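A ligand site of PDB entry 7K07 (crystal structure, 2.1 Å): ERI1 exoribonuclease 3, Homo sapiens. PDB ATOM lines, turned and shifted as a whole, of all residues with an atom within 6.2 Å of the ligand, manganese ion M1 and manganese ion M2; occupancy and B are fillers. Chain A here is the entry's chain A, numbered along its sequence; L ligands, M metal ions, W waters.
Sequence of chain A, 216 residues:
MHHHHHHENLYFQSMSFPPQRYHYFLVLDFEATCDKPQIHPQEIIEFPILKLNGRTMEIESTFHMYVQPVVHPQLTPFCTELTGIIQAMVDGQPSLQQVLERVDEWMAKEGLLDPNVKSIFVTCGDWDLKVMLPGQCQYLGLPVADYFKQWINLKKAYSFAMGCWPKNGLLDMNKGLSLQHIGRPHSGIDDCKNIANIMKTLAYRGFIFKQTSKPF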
ATOM      1  N   LEU A  28       7.442 -20.489  18.953  1.00  0.00           N
ATOM      2  CA  LEU A  28       8.575 -20.427  19.877  1.00  0.00           C
ATOM      3  C   LEU A  28       9.873 -20.400  19.091  1.00  0.00           C
ATOM      4  O   LEU A  28      10.015 -21.097  18.086  1.00  0.00           O
ATOM      5  CB  LEU A  28       8.557 -21.617  20.843  1.00  0.00           C
ATOM      6  CG  LEU A  28       9.676 -21.739  21.871  1.00  0.00           C
ATOM      7  CD1 LEU A  28       9.114 -22.326  23.139  1.00  0.00           C
ATOM      8  CD2 LEU A  28      10.813 -22.606  21.349  1.00  0.00           C
ATOM      9  N   ASP A  29      10.831 -19.594  19.553  1.00  0.00           N
ATOM     10  CA  ASP A  29      12.150 -19.562  18.924  1.00  0.00           C
ATOM     11  C   ASP A  29      13.181 -19.109  19.959  1.00  0.00           C
ATOM     12  O   ASP A  29      13.319 -17.913  20.212  1.00  0.00           O
ATOM     13  CB  ASP A  29      12.170 -18.643  17.716  1.00  0.00           C
ATOM     14  CG  ASP A  29      13.497 -18.708  16.970  1.00  0.00           C
ATOM     15  OD1 ASP A  29      13.732 -19.734  16.301  1.00  0.00           O
ATOM     16  OD2 ASP A  29      14.299 -17.757  17.069  1.00  0.00           O
ATOM     17  N   PHE A  30      13.920 -20.062  20.513  1.00  0.00           N
ATOM     18  CA  PHE A  30      14.970 -19.735  21.460  1.00  0.00           C
ATOM     19  C   PHE A  30      16.117 -18.981  20.785  1.00  0.00           C
ATOM     20  O   PHE A  30      16.400 -19.178  19.606  1.00  0.00           O
ATOM     21  CB  PHE A  30      15.546 -21.007  22.094  1.00  0.00           C
ATOM     22  CG  PHE A  30      14.550 -21.797  22.874  1.00  0.00           C
ATOM     23  CD1 PHE A  30      13.667 -21.157  23.735  1.00  0.00           C
ATOM     24  CD2 PHE A  30      14.491 -23.184  22.749  1.00  0.00           C
ATOM     25  CE1 PHE A  30      12.739 -21.887  24.463  1.00  0.00           C
ATOM     26  CE2 PHE A  30      13.576 -23.915  23.471  1.00  0.00           C
ATOM     27  CZ  PHE A  30      12.683 -23.260  24.342  1.00  0.00           C
ATOM     28  N   GLU A  31      16.751 -18.090  21.558  1.00  0.00           N
ATOM     29  CA  GLU A  31      18.143 -17.754  21.321  1.00  0.00           C
ATOM     30  C   GLU A  31      18.966 -18.315  22.477  1.00  0.00           C
ATOM     31  O   GLU A  31      18.460 -18.456  23.598  1.00  0.00           O
ATOM     32  CB  GLU A  31      18.371 -16.241  21.183  1.00  0.00           C
ATOM     33  CG  GLU A  31      17.530 -15.571  20.118  1.00  0.00           C
ATOM     34  CD  GLU A  31      17.742 -16.144  18.709  1.00  0.00           C
ATOM     35  OE1 GLU A  31      18.869 -16.594  18.395  1.00  0.00           O
ATOM     36  OE2 GLU A  31      16.767 -16.134  17.926  1.00  0.00           O
ATOM     37  N   ALA A  32      20.214 -18.677  22.186  1.00  0.00           N
ATOM     38  CA  ALA A  32      21.096 -19.303  23.153  1.00  0.00           C
ATOM     39  C   ALA A  32      22.469 -18.655  23.101  1.00  0.00           C
ATOM     40  O   ALA A  32      22.830 -18.013  22.111  1.00  0.00           O
ATOM     41  CB  ALA A  32      21.244 -20.818  22.898  1.00  0.00           C
ATOM     42  N   THR A  33      23.222 -18.818  24.189  1.00  0.00           N
ATOM     43  CA  THR A  33      24.650 -18.514  24.155  1.00  0.00           C
ATOM     44  C   THR A  33      25.306 -19.251  22.992  1.00  0.00           C
ATOM     45  O   THR A  33      24.930 -20.375  22.635  1.00  0.00           O
ATOM     46  CB  THR A  33      25.323 -18.941  25.470  1.00  0.00           C
ATOM     47  OG1 THR A  33      25.029 -20.312  25.743  1.00  0.00           O
ATOM     48  CG2 THR A  33      24.845 -18.091  26.637  1.00  0.00           C
ATOM     49  N   CYS A  34      26.302 -18.612  22.384  1.00  0.00           N
ATOM     50  CA  CYS A  34      27.018 -19.213  21.275  1.00  0.00           C
ATOM     51  C   CYS A  34      28.409 -18.589  21.195  1.00  0.00           C
ATOM     52  O   CYS A  34      28.744 -17.678  21.952  1.00  0.00           O
ATOM     53  CB  CYS A  34      26.237 -19.044  19.970  1.00  0.00           C
ATOM     54  SG  CYS A  34      25.696 -17.348  19.682  1.00  0.00           S
ATOM     55  N   ASP A  35      29.210 -19.101  20.271  1.00  0.00           N
ATOM     56  CA  ASP A  35      30.575 -18.644  20.077  1.00  0.00           C
ATOM     57  C   ASP A  35      31.101 -19.289  18.793  1.00  0.00           C
ATOM     58  O   ASP A  35      30.471 -20.186  18.234  1.00  0.00           O
ATOM     59  CB  ASP A  35      31.474 -18.990  21.271  1.00  0.00           C
ATOM     60  CG  ASP A  35      32.683 -18.052  21.387  1.00  0.00           C
ATOM     61  OD1 ASP A  35      32.872 -17.193  20.498  1.00  0.00           O
ATOM     62  OD2 ASP A  35      33.446 -18.178  22.372  1.00  0.00           O
ATOM     63  N   LYS A  36      32.249 -18.806  18.338  1.00  0.00           N
ATOM     64  CA  LYS A  36      32.980 -19.377  17.203  1.00  0.00           C
ATOM     65  C   LYS A  36      34.327 -19.873  17.704  1.00  0.00           C
ATOM     66  O   LYS A  36      35.170 -19.046  18.099  1.00  0.00           O
ATOM     67  CB  LYS A  36      33.181 -18.333  16.107  1.00  0.00           C
ATOM     68  CG  LYS A  36      32.718 -18.782  14.731  1.00  0.00           C
ATOM     69  CD  LYS A  36      31.211 -18.960  14.688  1.00  0.00           C
ATOM     70  CE  LYS A  36      30.776 -19.633  13.394  1.00  0.00           C
ATOM     71  NZ  LYS A  36      29.347 -20.037  13.427  1.00  0.00           N
ATOM     72  N   GLN A  38      31.655 -23.345  18.424  1.00  0.00           N
ATOM     73  CA  GLN A  38      30.472 -23.309  19.280  1.00  0.00           C
ATOM     74  C   GLN A  38      30.834 -23.464  20.757  1.00  0.00           C
ATOM     75  O   GLN A  38      31.752 -24.205  21.117  1.00  0.00           O
ATOM     76  CB  GLN A  38      29.485 -24.396  18.859  1.00  0.00           C
ATOM     77  CG  GLN A  38      28.074 -24.201  19.417  1.00  0.00           C
ATOM     78  CD  GLN A  38      27.526 -22.782  19.211  1.00  0.00           C
ATOM     79  OE1 GLN A  38      27.894 -21.866  19.935  1.00  0.00           O
ATOM     80  NE2 GLN A  38      26.640 -22.607  18.231  1.00  0.00           N
ATOM     81  N   GLN A  42      25.496 -24.992  25.357  1.00  0.00           N
ATOM     82  CA  GLN A  42      24.699 -23.809  25.103  1.00  0.00           C
ATOM     83  C   GLN A  42      23.618 -23.674  26.166  1.00  0.00           C
ATOM     84  O   GLN A  42      23.176 -24.660  26.771  1.00  0.00           O
ATOM     85  CB  GLN A  42      24.054 -23.875  23.724  1.00  0.00           C
ATOM     86  CG  GLN A  42      25.050 -23.827  22.577  1.00  0.00           C
ATOM     87  CD  GLN A  42      24.351 -23.718  21.239  1.00  0.00           C
ATOM     88  OE1 GLN A  42      24.063 -24.726  20.606  1.00  0.00           O
ATOM     89  NE2 GLN A  42      24.057 -22.492  20.822  1.00  0.00           N
ATOM     90  N   ILE A  45      18.992 -18.035  26.391  1.00  0.00           N
ATOM     91  CA  ILE A  45      19.028 -16.669  26.883  1.00  0.00           C
ATOM     92  C   ILE A  45      17.818 -15.851  26.474  1.00  0.00           C
ATOM     93  O   ILE A  45      17.668 -14.721  26.944  1.00  0.00           O
ATOM     94  CB  ILE A  45      20.317 -15.939  26.449  1.00  0.00           C
ATOM     95  CG1 ILE A  45      20.394 -15.857  24.927  1.00  0.00           C
ATOM     96  CG2 ILE A  45      21.549 -16.618  27.008  1.00  0.00           C
ATOM     97  CD1 ILE A  45      21.656 -15.176  24.433  1.00  0.00           C
ATOM     98  N   PHE A  78      30.634 -12.654  19.852  1.00  0.00           N
ATOM     99  CA  PHE A  78      29.917 -13.281  18.745  1.00  0.00           C
ATOM    100  C   PHE A  78      28.432 -13.390  19.049  1.00  0.00           C
ATOM    101  O   PHE A  78      27.578 -13.073  18.205  1.00  0.00           O
ATOM    102  CB  PHE A  78      30.491 -14.667  18.451  1.00  0.00           C
ATOM    103  CG  PHE A  78      29.751 -15.381  17.380  1.00  0.00           C
ATOM    104  CD1 PHE A  78      30.047 -15.157  16.046  1.00  0.00           C
ATOM    105  CD2 PHE A  78      28.734 -16.259  17.700  1.00  0.00           C
ATOM    106  CE1 PHE A  78      29.342 -15.800  15.054  1.00  0.00           C
ATOM    107  CE2 PHE A  78      28.007 -16.908  16.713  1.00  0.00           C
ATOM    108  CZ  PHE A  78      28.319 -16.672  15.379  1.00  0.00           C
ATOM    109  N   CYS A  79      28.098 -13.849  20.253  1.00  0.00           N
ATOM    110  CA  CYS A  79      26.700 -14.026  20.623  1.00  0.00           C
ATOM    111  C   CYS A  79      25.940 -12.707  20.557  1.00  0.00           C
ATOM    112  O   CYS A  79      24.803 -12.663  20.064  1.00  0.00           O
ATOM    113  CB  CYS A  79      26.608 -14.644  22.017  1.00  0.00           C
ATOM    114  SG  CYS A  79      24.941 -14.843  22.641  1.00  0.00           S
ATOM    115  N   LEU A  82      25.468 -11.674  16.953  1.00  0.00           N
ATOM    116  CA  LEU A  82      24.510 -12.513  16.255  1.00  0.00           C
ATOM    117  C   LEU A  82      23.085 -12.198  16.690  1.00  0.00           C
ATOM    118  O   LEU A  82      22.202 -11.976  15.847  1.00  0.00           O
ATOM    119  CB  LEU A  82      24.827 -13.989  16.503  1.00  0.00           C
ATOM    120  CG  LEU A  82      23.845 -14.948  15.828  1.00  0.00           C
ATOM    121  CD1 LEU A  82      24.008 -14.865  14.313  1.00  0.00           C
ATOM    122  CD2 LEU A  82      24.053 -16.361  16.338  1.00  0.00           C
ATOM    123  N   THR A  83      22.832 -12.160  18.003  1.00  0.00           N
ATOM    124  CA  THR A  83      21.461 -12.053  18.484  1.00  0.00           C
ATOM    125  C   THR A  83      21.014 -10.621  18.745  1.00  0.00           C
ATOM    126  O   THR A  83      19.806 -10.363  18.802  1.00  0.00           O
ATOM    127  CB  THR A  83      21.262 -12.865  19.779  1.00  0.00           C
ATOM    128  OG1 THR A  83      22.120 -12.344  20.800  1.00  0.00           O
ATOM    129  CG2 THR A  83      21.584 -14.363  19.541  1.00  0.00           C
ATOM    130  N   CYS A 124      10.749 -23.168  13.893  1.00  0.00           N
ATOM    131  CA  CYS A 124      11.468 -23.299  12.631  1.00  0.00           C
ATOM    132  C   CYS A 124      12.547 -24.360  12.824  1.00  0.00           C
ATOM    133  O   CYS A 124      13.613 -24.087  13.383  1.00  0.00           O
ATOM    134  CB  CYS A 124      12.060 -21.960  12.208  1.00  0.00           C
ATOM    135  SG  CYS A 124      12.822 -22.014  10.541  1.00  0.00           S
ATOM    136  N   TRP A 127      15.269 -28.109  16.276  1.00  0.00           N
ATOM    137  CA  TRP A 127      16.340 -27.929  17.252  1.00  0.00           C
ATOM    138  C   TRP A 127      15.821 -27.445  18.609  1.00  0.00           C
ATOM    139  O   TRP A 127      16.260 -27.942  19.659  1.00  0.00           O
ATOM    140  CB  TRP A 127      17.382 -26.949  16.694  1.00  0.00           C
ATOM    141  CG  TRP A 127      18.485 -26.610  17.641  1.00  0.00           C
ATOM    142  CD1 TRP A 127      19.593 -27.372  17.926  1.00  0.00           C
ATOM    143  CD2 TRP A 127      18.588 -25.434  18.449  1.00  0.00           C
ATOM    144  NE1 TRP A 127      20.373 -26.729  18.858  1.00  0.00           N
ATOM    145  CE2 TRP A 127      19.783 -25.541  19.192  1.00  0.00           C
ATOM    146  CE3 TRP A 127      17.781 -24.288  18.619  1.00  0.00           C
ATOM    147  CZ2 TRP A 127      20.203 -24.544  20.076  1.00  0.00           C
ATOM    148  CZ3 TRP A 127      18.202 -23.311  19.493  1.00  0.00           C
ATOM    149  CH2 TRP A 127      19.397 -23.451  20.221  1.00  0.00           C
ATOM    150  N   ASP A 128      14.876 -26.500  18.617  1.00  0.00           N
ATOM    151  CA  ASP A 128      14.467 -25.862  19.870  1.00  0.00           C
ATOM    152  C   ASP A 128      13.967 -26.870  20.888  1.00  0.00           C
ATOM    153  O   ASP A 128      14.425 -26.904  22.031  1.00  0.00           O
ATOM    154  CB  ASP A 128      13.386 -24.798  19.611  1.00  0.00           C
ATOM    155  CG  ASP A 128      13.820 -23.768  18.614  1.00  0.00           C
ATOM    156  OD1 ASP A 128      14.120 -22.625  19.029  1.00  0.00           O
ATOM    157  OD2 ASP A 128      13.906 -24.119  17.408  1.00  0.00           O
ATOM    158  N   HIS A 186      17.643 -13.153  13.646  1.00  0.00           N
ATOM    159  CA  HIS A 186      18.270 -13.753  14.816  1.00  0.00           C
ATOM    160  C   HIS A 186      17.871 -13.061  16.125  1.00  0.00           C
ATOM    161  O   HIS A 186      18.568 -13.216  17.142  1.00  0.00           O
ATOM    162  CB  HIS A 186      19.795 -13.782  14.665  1.00  0.00           C
ATOM    163  CG  HIS A 186      20.240 -14.368  13.355  1.00  0.00           C
ATOM    164  ND1 HIS A 186      20.347 -15.726  13.140  1.00  0.00           N
ATOM    165  CD2 HIS A 186      20.578 -13.763  12.194  1.00  0.00           C
ATOM    166  CE1 HIS A 186      20.742 -15.942  11.903  1.00  0.00           C
ATOM    167  NE2 HIS A 186      20.888 -14.773  11.299  1.00  0.00           N
ATOM    168  N   SER A 187      16.778 -12.319  16.124  1.00  0.00           N
ATOM    169  CA  SER A 187      16.077 -11.960  17.347  1.00  0.00           C
ATOM    170  C   SER A 187      14.984 -12.988  17.577  1.00  0.00           C
ATOM    171  O   SER A 187      14.195 -13.282  16.671  1.00  0.00           O
ATOM    172  CB  SER A 187      15.466 -10.557  17.258  1.00  0.00           C
ATOM    173  OG  SER A 187      14.540 -10.346  18.315  1.00  0.00           O
ATOM    174  N   GLY A 188      14.945 -13.543  18.798  1.00  0.00           N
ATOM    175  CA  GLY A 188      13.965 -14.591  19.073  1.00  0.00           C
ATOM    176  C   GLY A 188      12.539 -14.139  18.832  1.00  0.00           C
ATOM    177  O   GLY A 188      11.769 -14.812  18.137  1.00  0.00           O
ATOM    178  N   ASP A 191      11.982 -13.547  15.075  1.00  0.00           N
ATOM    179  CA  ASP A 191      11.830 -14.822  14.376  1.00  0.00           C
ATOM    180  C   ASP A 191      10.433 -15.388  14.589  1.00  0.00           C
ATOM    181  O   ASP A 191       9.811 -15.908  13.649  1.00  0.00           O
ATOM    182  CB  ASP A 191      12.907 -15.814  14.831  1.00  0.00           C
ATOM    183  CG  ASP A 191      14.299 -15.442  14.323  1.00  0.00           C
ATOM    184  OD1 ASP A 191      14.390 -14.655  13.353  1.00  0.00           O
ATOM    185  OD2 ASP A 191      15.302 -15.945  14.880  1.00  0.00           O
HETATM  186  P1  LIG L   1      18.224 -19.642  15.152  1.00  0.00           P
HETATM  187  O1  LIG L   1      18.002 -21.129  15.059  1.00  0.00           O
HETATM  188  O2  LIG L   1      16.995 -18.902  15.635  1.00  0.00           O
HETATM  189  O3  LIG L   1      18.858 -18.984  13.961  1.00  0.00           O
HETATM  190  O4  LIG L   1      19.309 -19.482  16.310  1.00  0.00           O
HETATM  191  C1  LIG L   1      19.288 -20.298  17.473  1.00  0.00           C
HETATM  192  C2  LIG L   1      20.620 -20.285  18.191  1.00  0.00           C
HETATM  193  O5  LIG L   1      21.581 -21.100  17.454  1.00  0.00           O
HETATM  194  C3  LIG L   1      21.313 -18.934  18.338  1.00  0.00           C
HETATM  195  O6  LIG L   1      20.811 -18.169  19.439  1.00  0.00           O
HETATM  196  C4  LIG L   1      22.773 -19.314  18.474  1.00  0.00           C
HETATM  197  O7  LIG L   1      23.051 -19.760  19.787  1.00  0.00           O
HETATM  198  C5  LIG L   1      22.864 -20.515  17.519  1.00  0.00           C
HETATM  199  N1  LIG L   1      23.238 -20.076  16.165  1.00  0.00           N
HETATM  200  C6  LIG L   1      22.381 -19.670  15.191  1.00  0.00           C
HETATM  201  N2  LIG L   1      23.059 -19.292  14.075  1.00  0.00           N
HETATM  202  C7  LIG L   1      24.366 -19.465  14.324  1.00  0.00           C
HETATM  203  C8  LIG L   1      25.620 -19.260  13.566  1.00  0.00           C
HETATM  204  N3  LIG L   1      25.579 -18.799  12.294  1.00  0.00           N
HETATM  205  N4  LIG L   1      26.776 -19.533  14.200  1.00  0.00           N
HETATM  206  C9  LIG L   1      26.817 -19.994  15.471  1.00  0.00           C
HETATM  207  N5  LIG L   1      25.723 -20.213  16.214  1.00  0.00           N
HETATM  208  C10 LIG L   1      24.482 -19.961  15.703  1.00  0.00           C
HETATM  209 MN    MN M   1      16.167 -17.155  16.206  1.00  0.00          MN
HETATM  210 MN    MN M   2      15.565 -20.704  15.679  1.00  0.00          MN
HETATM  211  O   HOH W   1      23.128 -23.993  17.908  1.00  0.00           O
HETATM  212  O   HOH W   2      14.932 -19.556  13.555  1.00  0.00           O
HETATM  213  O   HOH W   3      19.022 -20.518  11.801  1.00  0.00           O
HETATM  214  O   HOH W   4      15.969 -21.120  17.806  1.00  0.00           O
HETATM  215  O   HOH W   5      14.700 -22.734  15.703  1.00  0.00           O
HETATM  216  O   HOH W   6      18.384 -16.691  15.759  1.00  0.00           O
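The backbone NH of Ala 32 lies within hydrogen-bond range of an oxygen (O6) of the ligand (2.9 Å). O of Thr 33 lies within hydrogen-bond range of O7 of the ligand, at 3.5 Å. The backbone carbonyl oxygen (O) of Ala 32 is in hydrogen-bond range of an oxygen (O7) of the ligand. The side-chain amide nitrogen (NE2) of Gln 38 sits at hydrogen-bond distance from a nitrogen (N5) of the ligand. The side-chain sulfur (SG) of Cys 34 sits close to an oxygen (O7) of the ligand, at 3.6 Å. NZ of Lys 36 sits at hydrogen-bond distance from N4 of the ligand, 2.7 Å away. The side-chain amide nitrogen (NE2) of Gln 42 is in hydrogen-bond range of an oxygen (O7) of the ligand.
OD1 of Asp 128 is in hydrogen-bond range of N of Phe 30 (3.0 Å). The backbone NH of Asp 35 lies within hydrogen-bond range of the side-chain amide oxygen of Gln 38, at 3.1 Å. OE2 of Glu 31 sits close to N of Gly 188. The backbone NH of Ile 45 lies within hydrogen-bond range of the backbone carbonyl oxygen of Glu 31, at 2.9 Å. NE2 of Gln 42 sits at hydrogen-bond distance from O of Thr 33, 2.9 Å away. OG1 of Thr 83 is in hydrogen-bond range of O of Cys 79, at 2.8 Å.
Residues that only touch the ligand: Phe 30 (3.8 Å), Phe 78 (3.5 Å), Leu 82 (3.7 Å), Thr 83 (3.9 Å), Trp 127 (3.8 Å) and His 186 (3.7 Å). Hydrophobic or aromatic side chains that line the ligand: Ala 32, Phe 78, Leu 82 and Trp 127. Within 4 Å of the ligand: Asp 29, Phe 30, Glu 31, Ala 32, Thr 33, Cys 34, Lys 36, Gln 38, Gln 42, Phe 78, Leu 82, Thr 83, Trp 127, His 186 and Asp 191. The nearest printed residue that does not touch the ligand is Asp 35 (4.6 Å).
Residues that only touch manganese ion M1: Phe 30. Within 4 Å of manganese ion M1: Asp 29, Phe 30, Glu 31 and Asp 191. The nearest printed residue that does not touch manganese ion M1 is His 186 (4.2 Å).
Of the 23 residues printed, 1 comes within 4 Å of manganese ion M2.
Manganese ion M1 is bound by the side-chain carboxylate of Asp 191 (2.0 Å), an oxygen (O2) of the ligand (2.0 Å), the side-chain carboxylate of Glu 31 (2.1 Å), the side-chain carboxylate of Asp 29 (2.1 Å) and water W6 (2.3 Å).
OD1 of Asp 29 binds manganese ion M2 (2.2 Å). Water W4 binds manganese ion M2 (2.2 Å). Manganese ion M2 is bound by water W5 (2.2 Å). An oxygen (O2) of the ligand is bound to manganese ion M2 (2.3 Å). Water W2 is bound to manganese ion M2 (2.5 Å). An oxygen (O1) of the ligand binds manganese ion M2, at 2.6 Å.
Water W6 lies within hydrogen-bond range of OE1 of Glu 31, O3 of the ligand and ND1 of His 186. Water W4 lies within hydrogen-bond range of OD1 of Asp 128 (2.7 Å) and O of Phe 30 (2.7 Å). Water W5 bridges the backbone carbonyl oxygen (O) of Cys 124 (2.9 Å) and the side-chain carboxylate (OD1) of Asp 128 (3.4 Å). Water W1 bridges the side-chain amide oxygen of Gln 42 (2.9 Å) and an oxygen (O5) of the ligand (3.3 Å).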
